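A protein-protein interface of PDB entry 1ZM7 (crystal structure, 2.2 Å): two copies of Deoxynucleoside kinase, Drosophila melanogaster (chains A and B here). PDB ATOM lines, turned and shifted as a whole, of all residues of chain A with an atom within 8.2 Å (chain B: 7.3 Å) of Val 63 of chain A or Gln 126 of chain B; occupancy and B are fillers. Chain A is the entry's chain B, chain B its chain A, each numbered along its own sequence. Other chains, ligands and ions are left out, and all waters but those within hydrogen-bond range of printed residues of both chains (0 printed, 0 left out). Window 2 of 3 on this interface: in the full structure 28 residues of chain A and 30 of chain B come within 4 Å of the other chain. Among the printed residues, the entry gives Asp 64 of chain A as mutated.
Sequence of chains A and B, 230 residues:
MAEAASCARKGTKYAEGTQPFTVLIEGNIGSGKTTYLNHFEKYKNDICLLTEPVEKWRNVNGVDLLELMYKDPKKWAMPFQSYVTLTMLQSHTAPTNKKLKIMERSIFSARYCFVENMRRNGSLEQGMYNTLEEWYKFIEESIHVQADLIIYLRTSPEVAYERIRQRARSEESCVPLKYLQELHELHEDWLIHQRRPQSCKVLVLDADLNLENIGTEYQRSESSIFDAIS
The side-chain sulfur (SD) of Met 128 of chain B lies within hydrogen-bond range of the backbone NH (N) of Glu 125 of chain B (3.6 Å). The backbone carbonyl oxygen (O) of Gln 126 of chain B sits at hydrogen-bond distance from the side-chain amide nitrogen (ND2) of Asn 130 of chain B, at 3.0 Å. The side-chain hydroxyl (OG1) of Thr 131 of chain B sits at hydrogen-bond distance from the backbone carbonyl oxygen (O) of Gly 127 of chain B, at 2.8 Å. N of Leu 65 of chain A is in hydrogen-bond range of O of Trp 57 of chain A (3.2 Å).
The side-chain carboxylate (OE2) of Glu 125 of chain B lies within salt-bridge range of the side-chain amino group (NZ) of Lys 75 of chain A, at 2.7 Å.
No position is printed for both chains. Of the 9 pairs that touch across the chains among the printed residues, none has its exchanged pair printed and touching as well.
Of chain A, only Val 63 comes within 4 Å of Gln 126 of chain B. No residue of chain B comes within 4 Å of Gly 62 of chain A. Of the printed residues of chain A, Asn 130 of chain B touches Asn 61 (3.6 Å). Of the printed residues of chain A, Thr 131 of chain B touches Leu 65 and Tyr 83. Of the printed residues of chain A, Met 128 of chain B touches Lys 75 and Trp 76. Printed residues of chain A within 4 Å of Glu 125 of chain B: Lys 75 (2.7 Å) and Trp 76 (3.6 Å). Glu 55 of chain A touches none of the printed residues of chain B. Asn 59 of chain A touches none of the printed residues of chain B. The nearest printed residue of chain B that does not touch Val 63 of chain A is Asn 130 of chain B (4.01 Å).
Of the 18 printed residues of chain A, 6 touch a printed residue of chain B. Hydrophobic or aromatic side chains of chain A that line the printed part of chain B: Val 63, Leu 65, Trp 76 and Tyr 83. Hydrophobic or aromatic side chains of chain B within 4 Å of the printed part of chain A: Met 128. Among the printed residues, Asp or Glu carboxylates within 4 Å of a Lys or Arg side-chain nitrogen of the other chain: Lys 75 of chain A with Glu 125 of chain B.
Among the printed residues, merely in contact across the chains: Asn 61 of chain A with Asn 130 of chain B, Trp 76 of chain A with Glu 125 of chain B, Val 63 of chain A with Gln 126 of chain B, Lys 75 of chain A with Met 128 of chain B, Leu 65 of chain A with Thr 131 of chain B, Tyr 83 of chain A with Thr 131 of chain B, Trp 76 of chain A with Met 128 of chain B and Trp 76 of chain A with Gly 127 of chain B.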
ATOM      1  N   GLU A  55     -17.259 -12.178  17.338  1.00  0.00           N
ATOM      2  CA  GLU A  55     -17.966 -13.378  16.879  1.00  0.00           C
ATOM      3  C   GLU A  55     -17.581 -14.635  17.680  1.00  0.00           C
ATOM      4  O   GLU A  55     -18.418 -15.476  17.943  1.00  0.00           O
ATOM      5  CB  GLU A  55     -17.824 -13.582  15.350  1.00  0.00           C
ATOM      6  CG  GLU A  55     -18.582 -12.521  14.535  1.00  0.00           C
ATOM      7  CD  GLU A  55     -20.048 -12.357  14.951  1.00  0.00           C
ATOM      8  OE1 GLU A  55     -20.829 -13.350  14.879  1.00  0.00           O
ATOM      9  OE2 GLU A  55     -20.442 -11.231  15.353  1.00  0.00           O
ATOM     10  N   LYS A  56     -16.327 -14.733  18.092  1.00  0.00           N
ATOM     11  CA  LYS A  56     -15.912 -15.793  18.998  1.00  0.00           C
ATOM     12  C   LYS A  56     -16.592 -15.682  20.366  1.00  0.00           C
ATOM     13  O   LYS A  56     -17.030 -16.679  20.920  1.00  0.00           O
ATOM     14  CB  LYS A  56     -14.399 -15.775  19.177  1.00  0.00           C
ATOM     15  CG  LYS A  56     -13.637 -16.243  17.919  1.00  0.00           C
ATOM     16  CD  LYS A  56     -12.182 -15.777  17.992  1.00  0.00           C
ATOM     17  CE  LYS A  56     -11.399 -16.154  16.723  1.00  0.00           C
ATOM     18  NZ  LYS A  56     -10.445 -15.057  16.389  1.00  0.00           N
ATOM     19  N   TRP A  57     -16.688 -14.458  20.891  1.00  0.00           N
ATOM     20  CA  TRP A  57     -17.183 -14.232  22.248  1.00  0.00           C
ATOM     21  C   TRP A  57     -18.673 -14.459  22.307  1.00  0.00           C
ATOM     22  O   TRP A  57     -19.218 -14.716  23.366  1.00  0.00           O
ATOM     23  CB  TRP A  57     -16.837 -12.809  22.734  1.00  0.00           C
ATOM     24  CG  TRP A  57     -15.407 -12.431  22.497  1.00  0.00           C
ATOM     25  CD1 TRP A  57     -14.332 -13.276  22.415  1.00  0.00           C
ATOM     26  CD2 TRP A  57     -14.887 -11.115  22.314  1.00  0.00           C
ATOM     27  NE1 TRP A  57     -13.183 -12.564  22.173  1.00  0.00           N
ATOM     28  CE2 TRP A  57     -13.494 -11.234  22.105  1.00  0.00           C
ATOM     29  CE3 TRP A  57     -15.460  -9.836  22.294  1.00  0.00           C
ATOM     30  CZ2 TRP A  57     -12.671 -10.138  21.876  1.00  0.00           C
ATOM     31  CZ3 TRP A  57     -14.636  -8.743  22.051  1.00  0.00           C
ATOM     32  CH2 TRP A  57     -13.257  -8.901  21.858  1.00  0.00           C
ATOM     33  N   ARG A  58     -19.332 -14.379  21.157  1.00  0.00           N
ATOM     34  CA  ARG A  58     -20.763 -14.601  21.102  1.00  0.00           C
ATOM     35  C   ARG A  58     -21.120 -16.071  20.904  1.00  0.00           C
ATOM     36  O   ARG A  58     -22.285 -16.427  20.957  1.00  0.00           O
ATOM     37  CB  ARG A  58     -21.386 -13.821  19.953  1.00  0.00           C
ATOM     38  CG  ARG A  58     -21.288 -12.345  20.107  1.00  0.00           C
ATOM     39  CD  ARG A  58     -21.686 -11.619  18.828  1.00  0.00           C
ATOM     40  NE  ARG A  58     -23.134 -11.426  18.753  1.00  0.00           N
ATOM     41  CZ  ARG A  58     -23.783 -10.977  17.673  1.00  0.00           C
ATOM     42  NH1 ARG A  58     -23.124 -10.681  16.550  1.00  0.00           N
ATOM     43  NH2 ARG A  58     -25.097 -10.811  17.723  1.00  0.00           N
ATOM     44  N   ASN A  59     -20.131 -16.922  20.666  1.00  0.00           N
ATOM     45  CA  ASN A  59     -20.420 -18.326  20.399  1.00  0.00           C
ATOM     46  C   ASN A  59     -19.242 -19.204  20.780  1.00  0.00           C
ATOM     47  O   ASN A  59     -18.347 -19.443  19.970  1.00  0.00           O
ATOM     48  CB  ASN A  59     -20.825 -18.511  18.909  1.00  0.00           C
ATOM     49  CG  ASN A  59     -20.982 -19.983  18.502  1.00  0.00           C
ATOM     50  OD1 ASN A  59     -21.101 -20.877  19.346  1.00  0.00           O
ATOM     51  ND2 ASN A  59     -20.979 -20.235  17.194  1.00  0.00           N
ATOM     52  N   VAL A  60     -19.212 -19.647  22.025  1.00  0.00           N
ATOM     53  CA  VAL A  60     -18.128 -20.475  22.522  1.00  0.00           C
ATOM     54  C   VAL A  60     -18.733 -21.870  22.670  1.00  0.00           C
ATOM     55  O   VAL A  60     -19.491 -22.126  23.630  1.00  0.00           O
ATOM     56  CB  VAL A  60     -17.598 -19.978  23.905  1.00  0.00           C
ATOM     57  CG1 VAL A  60     -16.355 -20.778  24.327  1.00  0.00           C
ATOM     58  CG2 VAL A  60     -17.288 -18.471  23.886  1.00  0.00           C
ATOM     59  N   ASN A  61     -18.453 -22.744  21.696  1.00  0.00           N
ATOM     60  CA  ASN A  61     -19.173 -24.011  21.548  1.00  0.00           C
ATOM     61  C   ASN A  61     -20.678 -23.868  21.743  1.00  0.00           C
ATOM     62  O   ASN A  61     -21.282 -24.668  22.438  1.00  0.00           O
ATOM     63  CB  ASN A  61     -18.637 -25.073  22.529  1.00  0.00           C
ATOM     64  CG  ASN A  61     -17.143 -24.990  22.725  1.00  0.00           C
ATOM     65  OD1 ASN A  61     -16.354 -25.254  21.795  1.00  0.00           O
ATOM     66  ND2 ASN A  61     -16.725 -24.605  23.939  1.00  0.00           N
ATOM     67  N   GLY A  62     -21.288 -22.821  21.197  1.00  0.00           N
ATOM     68  CA  GLY A  62     -22.717 -22.638  21.399  1.00  0.00           C
ATOM     69  C   GLY A  62     -23.151 -21.754  22.557  1.00  0.00           C
ATOM     70  O   GLY A  62     -24.327 -21.435  22.653  1.00  0.00           O
ATOM     71  N   VAL A  63     -22.227 -21.347  23.424  1.00  0.00           N
ATOM     72  CA  VAL A  63     -22.558 -20.464  24.551  1.00  0.00           C
ATOM     73  C   VAL A  63     -22.256 -19.003  24.196  1.00  0.00           C
ATOM     74  O   VAL A  63     -21.156 -18.666  23.757  1.00  0.00           O
ATOM     75  CB  VAL A  63     -21.778 -20.869  25.837  1.00  0.00           C
ATOM     76  CG1 VAL A  63     -22.007 -19.865  26.965  1.00  0.00           C
ATOM     77  CG2 VAL A  63     -22.206 -22.255  26.289  1.00  0.00           C
ATOM     78  N   ASP A  64     -23.248 -18.140  24.375  1.00  0.00           N
ATOM     79  CA  ASP A  64     -23.071 -16.710  24.129  1.00  0.00           C
ATOM     80  C   ASP A  64     -22.532 -16.013  25.391  1.00  0.00           C
ATOM     81  O   ASP A  64     -23.312 -15.528  26.218  1.00  0.00           O
ATOM     82  CB  ASP A  64     -24.387 -16.100  23.663  1.00  0.00           C
ATOM     83  CG  ASP A  64     -24.217 -14.723  23.045  1.00  0.00           C
ATOM     84  OD1 ASP A  64     -23.253 -13.987  23.391  1.00  0.00           O
ATOM     85  OD2 ASP A  64     -25.038 -14.268  22.211  1.00  0.00           O
ATOM     86  N   LEU A  65     -21.199 -15.982  25.544  1.00  0.00           N
ATOM     87  CA  LEU A  65     -20.575 -15.374  26.729  1.00  0.00           C
ATOM     88  C   LEU A  65     -20.848 -13.878  26.806  1.00  0.00           C
ATOM     89  O   LEU A  65     -21.016 -13.332  27.905  1.00  0.00           O
ATOM     90  CB  LEU A  65     -19.056 -15.586  26.771  1.00  0.00           C
ATOM     91  CG  LEU A  65     -18.431 -16.904  27.237  1.00  0.00           C
ATOM     92  CD1 LEU A  65     -16.905 -16.750  27.226  1.00  0.00           C
ATOM     93  CD2 LEU A  65     -18.922 -17.360  28.617  1.00  0.00           C
ATOM     94  N   LEU A  66     -20.868 -13.219  25.649  1.00  0.00           N
ATOM     95  CA  LEU A  66     -21.162 -11.786  25.596  1.00  0.00           C
ATOM     96  C   LEU A  66     -22.531 -11.490  26.235  1.00  0.00           C
ATOM     97  O   LEU A  66     -22.652 -10.599  27.082  1.00  0.00           O
ATOM     98  CB  LEU A  66     -21.118 -11.268  24.144  1.00  0.00           C
ATOM     99  CG  LEU A  66     -21.280  -9.752  23.955  1.00  0.00           C
ATOM    100  CD1 LEU A  66     -20.121  -8.960  24.602  1.00  0.00           C
ATOM    101  CD2 LEU A  66     -21.408  -9.403  22.484  1.00  0.00           C
ATOM    102  N   GLU A  67     -23.540 -12.249  25.833  1.00  0.00           N
ATOM    103  CA  GLU A  67     -24.881 -12.119  26.375  1.00  0.00           C
ATOM    104  C   GLU A  67     -24.915 -12.347  27.886  1.00  0.00           C
ATOM    105  O   GLU A  67     -25.509 -11.558  28.613  1.00  0.00           O
ATOM    106  CB  GLU A  67     -25.798 -13.118  25.693  1.00  0.00           C
ATOM    107  CG  GLU A  67     -27.083 -13.407  26.450  1.00  0.00           C
ATOM    108  CD  GLU A  67     -28.241 -12.602  25.917  1.00  0.00           C
ATOM    109  OE1 GLU A  67     -28.296 -11.372  26.189  1.00  0.00           O
ATOM    110  OE2 GLU A  67     -29.096 -13.207  25.213  1.00  0.00           O
ATOM    111  N   LEU A  68     -24.307 -13.439  28.347  1.00  0.00           N
ATOM    112  CA  LEU A  68     -24.288 -13.745  29.775  1.00  0.00           C
ATOM    113  C   LEU A  68     -23.624 -12.646  30.582  1.00  0.00           C
ATOM    114  O   LEU A  68     -24.055 -12.349  31.687  1.00  0.00           O
ATOM    115  CB  LEU A  68     -23.593 -15.068  30.059  1.00  0.00           C
ATOM    116  CG  LEU A  68     -24.376 -16.269  29.542  1.00  0.00           C
ATOM    117  CD1 LEU A  68     -23.410 -17.430  29.360  1.00  0.00           C
ATOM    118  CD2 LEU A  68     -25.510 -16.644  30.512  1.00  0.00           C
ATOM    119  N   LYS A  75     -21.396 -12.184  37.919  1.00  0.00           N
ATOM    120  CA  LYS A  75     -21.023 -13.581  37.812  1.00  0.00           C
ATOM    121  C   LYS A  75     -20.184 -13.862  36.538  1.00  0.00           C
ATOM    122  O   LYS A  75     -19.310 -14.728  36.544  1.00  0.00           O
ATOM    123  CB  LYS A  75     -22.315 -14.402  37.824  1.00  0.00           C
ATOM    124  CG  LYS A  75     -22.146 -15.886  37.707  1.00  0.00           C
ATOM    125  CD  LYS A  75     -23.532 -16.563  37.679  1.00  0.00           C
ATOM    126  CE  LYS A  75     -23.403 -18.056  37.821  1.00  0.00           C
ATOM    127  NZ  LYS A  75     -24.684 -18.774  37.517  1.00  0.00           N
ATOM    128  N   TRP A  76     -20.460 -13.134  35.462  1.00  0.00           N
ATOM    129  CA  TRP A  76     -19.937 -13.492  34.140  1.00  0.00           C
ATOM    130  C   TRP A  76     -18.859 -12.578  33.589  1.00  0.00           C
ATOM    131  O   TRP A  76     -18.196 -12.943  32.627  1.00  0.00           O
ATOM    132  CB  TRP A  76     -21.075 -13.666  33.095  1.00  0.00           C
ATOM    133  CG  TRP A  76     -21.824 -14.940  33.299  1.00  0.00           C
ATOM    134  CD1 TRP A  76     -23.006 -15.106  33.971  1.00  0.00           C
ATOM    135  CD2 TRP A  76     -21.433 -16.250  32.855  1.00  0.00           C
ATOM    136  NE1 TRP A  76     -23.365 -16.433  33.978  1.00  0.00           N
ATOM    137  CE2 TRP A  76     -22.423 -17.157  33.301  1.00  0.00           C
ATOM    138  CE3 TRP A  76     -20.345 -16.749  32.133  1.00  0.00           C
ATOM    139  CZ2 TRP A  76     -22.370 -18.522  33.025  1.00  0.00           C
ATOM    140  CZ3 TRP A  76     -20.275 -18.110  31.881  1.00  0.00           C
ATOM    141  CH2 TRP A  76     -21.287 -18.978  32.304  1.00  0.00           C
ATOM    142  N   TYR A  83     -11.891 -15.034  28.775  1.00  0.00           N
ATOM    143  CA  TYR A  83     -11.982 -15.574  27.424  1.00  0.00           C
ATOM    144  C   TYR A  83     -11.528 -14.535  26.387  1.00  0.00           C
ATOM    145  O   TYR A  83     -10.818 -14.876  25.432  1.00  0.00           O
ATOM    146  CB  TYR A  83     -13.386 -16.099  27.108  1.00  0.00           C
ATOM    147  CG  TYR A  83     -13.443 -16.871  25.812  1.00  0.00           C
ATOM    148  CD1 TYR A  83     -12.798 -18.091  25.680  1.00  0.00           C
ATOM    149  CD2 TYR A  83     -14.102 -16.351  24.700  1.00  0.00           C
ATOM    150  CE1 TYR A  83     -12.827 -18.808  24.455  1.00  0.00           C
ATOM    151  CE2 TYR A  83     -14.134 -17.051  23.489  1.00  0.00           C
ATOM    152  CZ  TYR A  83     -13.494 -18.274  23.387  1.00  0.00           C
ATOM    153  OH  TYR A  83     -13.532 -18.944  22.194  1.00  0.00           O
ATOM    154  N   GLU A 171     -27.203  -8.690  22.074  1.00  0.00           N
ATOM    155  CA  GLU A 171     -26.497  -8.680  23.362  1.00  0.00           C
ATOM    156  C   GLU A 171     -26.296  -7.252  23.870  1.00  0.00           C
ATOM    157  O   GLU A 171     -26.281  -7.014  25.075  1.00  0.00           O
ATOM    158  CB  GLU A 171     -25.139  -9.393  23.262  1.00  0.00           C
ATOM    159  CG  GLU A 171     -25.195 -10.869  22.861  1.00  0.00           C
ATOM    160  CD  GLU A 171     -25.106 -11.096  21.353  1.00  0.00           C
ATOM    161  OE1 GLU A 171     -25.405 -10.154  20.573  1.00  0.00           O
ATOM    162  OE2 GLU A 171     -24.743 -12.229  20.943  1.00  0.00           O
ATOM    163  N   ARG B 119     -17.167 -28.646  37.574  1.00  0.00           N
ATOM    164  CA  ARG B 119     -18.147 -28.804  36.501  1.00  0.00           C
ATOM    165  C   ARG B 119     -19.268 -29.800  36.905  1.00  0.00           C
ATOM    166  O   ARG B 119     -20.446 -29.493  36.768  1.00  0.00           O
ATOM    167  CB  ARG B 119     -17.466 -29.258  35.211  1.00  0.00           C
ATOM    168  CG  ARG B 119     -18.452 -29.448  34.046  1.00  0.00           C
ATOM    169  CD  ARG B 119     -17.868 -30.171  32.838  1.00  0.00           C
ATOM    170  NE  ARG B 119     -17.626 -31.593  33.063  1.00  0.00           N
ATOM    171  CZ  ARG B 119     -18.563 -32.555  32.970  1.00  0.00           C
ATOM    172  NH1 ARG B 119     -19.811 -32.246  32.685  1.00  0.00           N
ATOM    173  NH2 ARG B 119     -18.245 -33.822  33.175  1.00  0.00           N
ATOM    174  N   GLY B 122     -21.834 -28.499  39.527  1.00  0.00           N
ATOM    175  CA  GLY B 122     -22.538 -27.270  39.192  1.00  0.00           C
ATOM    176  C   GLY B 122     -21.927 -25.958  39.677  1.00  0.00           C
ATOM    177  O   GLY B 122     -22.535 -24.894  39.493  1.00  0.00           O
ATOM    178  N   LEU B 124     -19.154 -24.597  38.495  1.00  0.00           N
ATOM    179  CA  LEU B 124     -18.779 -23.951  37.244  1.00  0.00           C
ATOM    180  C   LEU B 124     -19.887 -24.180  36.240  1.00  0.00           C
ATOM    181  O   LEU B 124     -20.182 -25.329  35.910  1.00  0.00           O
ATOM    182  CB  LEU B 124     -17.470 -24.546  36.675  1.00  0.00           C
ATOM    183  CG  LEU B 124     -16.183 -24.319  37.470  1.00  0.00           C
ATOM    184  CD1 LEU B 124     -15.042 -25.128  36.856  1.00  0.00           C
ATOM    185  CD2 LEU B 124     -15.809 -22.840  37.566  1.00  0.00           C
ATOM    186  N   GLU B 125     -20.504 -23.105  35.762  1.00  0.00           N
ATOM    187  CA  GLU B 125     -21.411 -23.206  34.626  1.00  0.00           C
ATOM    188  C   GLU B 125     -20.634 -23.630  33.384  1.00  0.00           C
ATOM    189  O   GLU B 125     -19.412 -23.461  33.305  1.00  0.00           O
ATOM    190  CB  GLU B 125     -22.104 -21.873  34.337  1.00  0.00           C
ATOM    191  CG  GLU B 125     -22.813 -21.257  35.530  1.00  0.00           C
ATOM    192  CD  GLU B 125     -24.229 -21.774  35.717  1.00  0.00           C
ATOM    193  OE1 GLU B 125     -24.691 -22.614  34.893  1.00  0.00           O
ATOM    194  OE2 GLU B 125     -24.880 -21.341  36.697  1.00  0.00           O
ATOM    195  N   GLN B 126     -21.362 -24.157  32.405  1.00  0.00           N
ATOM    196  CA  GLN B 126     -20.730 -24.679  31.196  1.00  0.00           C
ATOM    197  C   GLN B 126     -19.764 -23.661  30.592  1.00  0.00           C
ATOM    198  O   GLN B 126     -18.630 -24.003  30.276  1.00  0.00           O
ATOM    199  CB  GLN B 126     -21.804 -25.111  30.181  1.00  0.00           C
ATOM    200  CG  GLN B 126     -21.247 -25.968  29.060  1.00  0.00           C
ATOM    201  CD  GLN B 126     -22.058 -25.808  27.780  1.00  0.00           C
ATOM    202  OE1 GLN B 126     -23.268 -25.684  27.827  1.00  0.00           O
ATOM    203  NE2 GLN B 126     -21.388 -25.772  26.654  1.00  0.00           N
ATOM    204  N   GLY B 127     -20.199 -22.411  30.453  1.00  0.00           N
ATOM    205  CA  GLY B 127     -19.376 -21.374  29.859  1.00  0.00           C
ATOM    206  C   GLY B 127     -18.077 -21.063  30.620  1.00  0.00           C
ATOM    207  O   GLY B 127     -17.065 -20.666  30.020  1.00  0.00           O
ATOM    208  N   MET B 128     -18.102 -21.253  31.934  1.00  0.00           N
ATOM    209  CA  MET B 128     -16.922 -21.049  32.779  1.00  0.00           C
ATOM    210  C   MET B 128     -15.967 -22.213  32.594  1.00  0.00           C
ATOM    211  O   MET B 128     -14.787 -22.035  32.434  1.00  0.00           O
ATOM    212  CB  MET B 128     -17.358 -20.987  34.248  1.00  0.00           C
ATOM    213  CG  MET B 128     -18.033 -19.667  34.605  1.00  0.00           C
ATOM    214  SD  MET B 128     -18.864 -19.881  36.161  1.00  0.00           S
ATOM    215  CE  MET B 128     -19.901 -18.397  36.192  1.00  0.00           C
ATOM    216  N   TYR B 129     -16.527 -23.423  32.576  1.00  0.00           N
ATOM    217  CA  TYR B 129     -15.754 -24.612  32.313  1.00  0.00           C
ATOM    218  C   TYR B 129     -15.094 -24.540  30.928  1.00  0.00           C
ATOM    219  O   TYR B 129     -13.919 -24.848  30.792  1.00  0.00           O
ATOM    220  CB  TYR B 129     -16.645 -25.851  32.428  1.00  0.00           C
ATOM    221  CG  TYR B 129     -15.988 -27.122  31.901  1.00  0.00           C
ATOM    222  CD1 TYR B 129     -15.019 -27.793  32.647  1.00  0.00           C
ATOM    223  CD2 TYR B 129     -16.352 -27.653  30.657  1.00  0.00           C
ATOM    224  CE1 TYR B 129     -14.418 -28.975  32.182  1.00  0.00           C
ATOM    225  CE2 TYR B 129     -15.751 -28.839  30.162  1.00  0.00           C
ATOM    226  CZ  TYR B 129     -14.792 -29.493  30.935  1.00  0.00           C
ATOM    227  OH  TYR B 129     -14.208 -30.653  30.475  1.00  0.00           O
ATOM    228  N   ASN B 130     -15.851 -24.129  29.911  1.00  0.00           N
ATOM    229  CA  ASN B 130     -15.292 -24.037  28.551  1.00  0.00           C
ATOM    230  C   ASN B 130     -14.144 -23.021  28.488  1.00  0.00           C
ATOM    231  O   ASN B 130     -13.122 -23.271  27.840  1.00  0.00           O
ATOM    232  CB  ASN B 130     -16.357 -23.624  27.517  1.00  0.00           C
ATOM    233  CG  ASN B 130     -17.543 -24.592  27.428  1.00  0.00           C
ATOM    234  OD1 ASN B 130     -17.389 -25.825  27.429  1.00  0.00           O
ATOM    235  ND2 ASN B 130     -18.741 -24.018  27.285  1.00  0.00           N
ATOM    236  N   THR B 131     -14.303 -21.877  29.163  1.00  0.00           N
ATOM    237  CA  THR B 131     -13.234 -20.870  29.220  1.00  0.00           C
ATOM    238  C   THR B 131     -11.947 -21.451  29.837  1.00  0.00           C
ATOM    239  O   THR B 131     -10.875 -21.312  29.271  1.00  0.00           O
ATOM    240  CB  THR B 131     -13.726 -19.630  29.987  1.00  0.00           C
ATOM    241  OG1 THR B 131     -14.843 -19.080  29.273  1.00  0.00           O
ATOM    242  CG2 THR B 131     -12.681 -18.508  29.950  1.00  0.00           C
ATOM    243  N   LEU B 132     -12.065 -22.119  30.978  1.00  0.00           N
ATOM    244  CA  LEU B 132     -10.910 -22.757  31.606  1.00  0.00           C
ATOM    245  C   LEU B 132     -10.270 -23.792  30.670  1.00  0.00           C
ATOM    246  O   LEU B 132      -9.044 -23.813  30.506  1.00  0.00           O
ATOM    247  CB  LEU B 132     -11.266 -23.383  32.968  1.00  0.00           C
ATOM    248  CG  LEU B 132     -11.744 -22.394  34.056  1.00  0.00           C
ATOM    249  CD1 LEU B 132     -12.448 -23.103  35.217  1.00  0.00           C
ATOM    250  CD2 LEU B 132     -10.571 -21.522  34.590  1.00  0.00           C
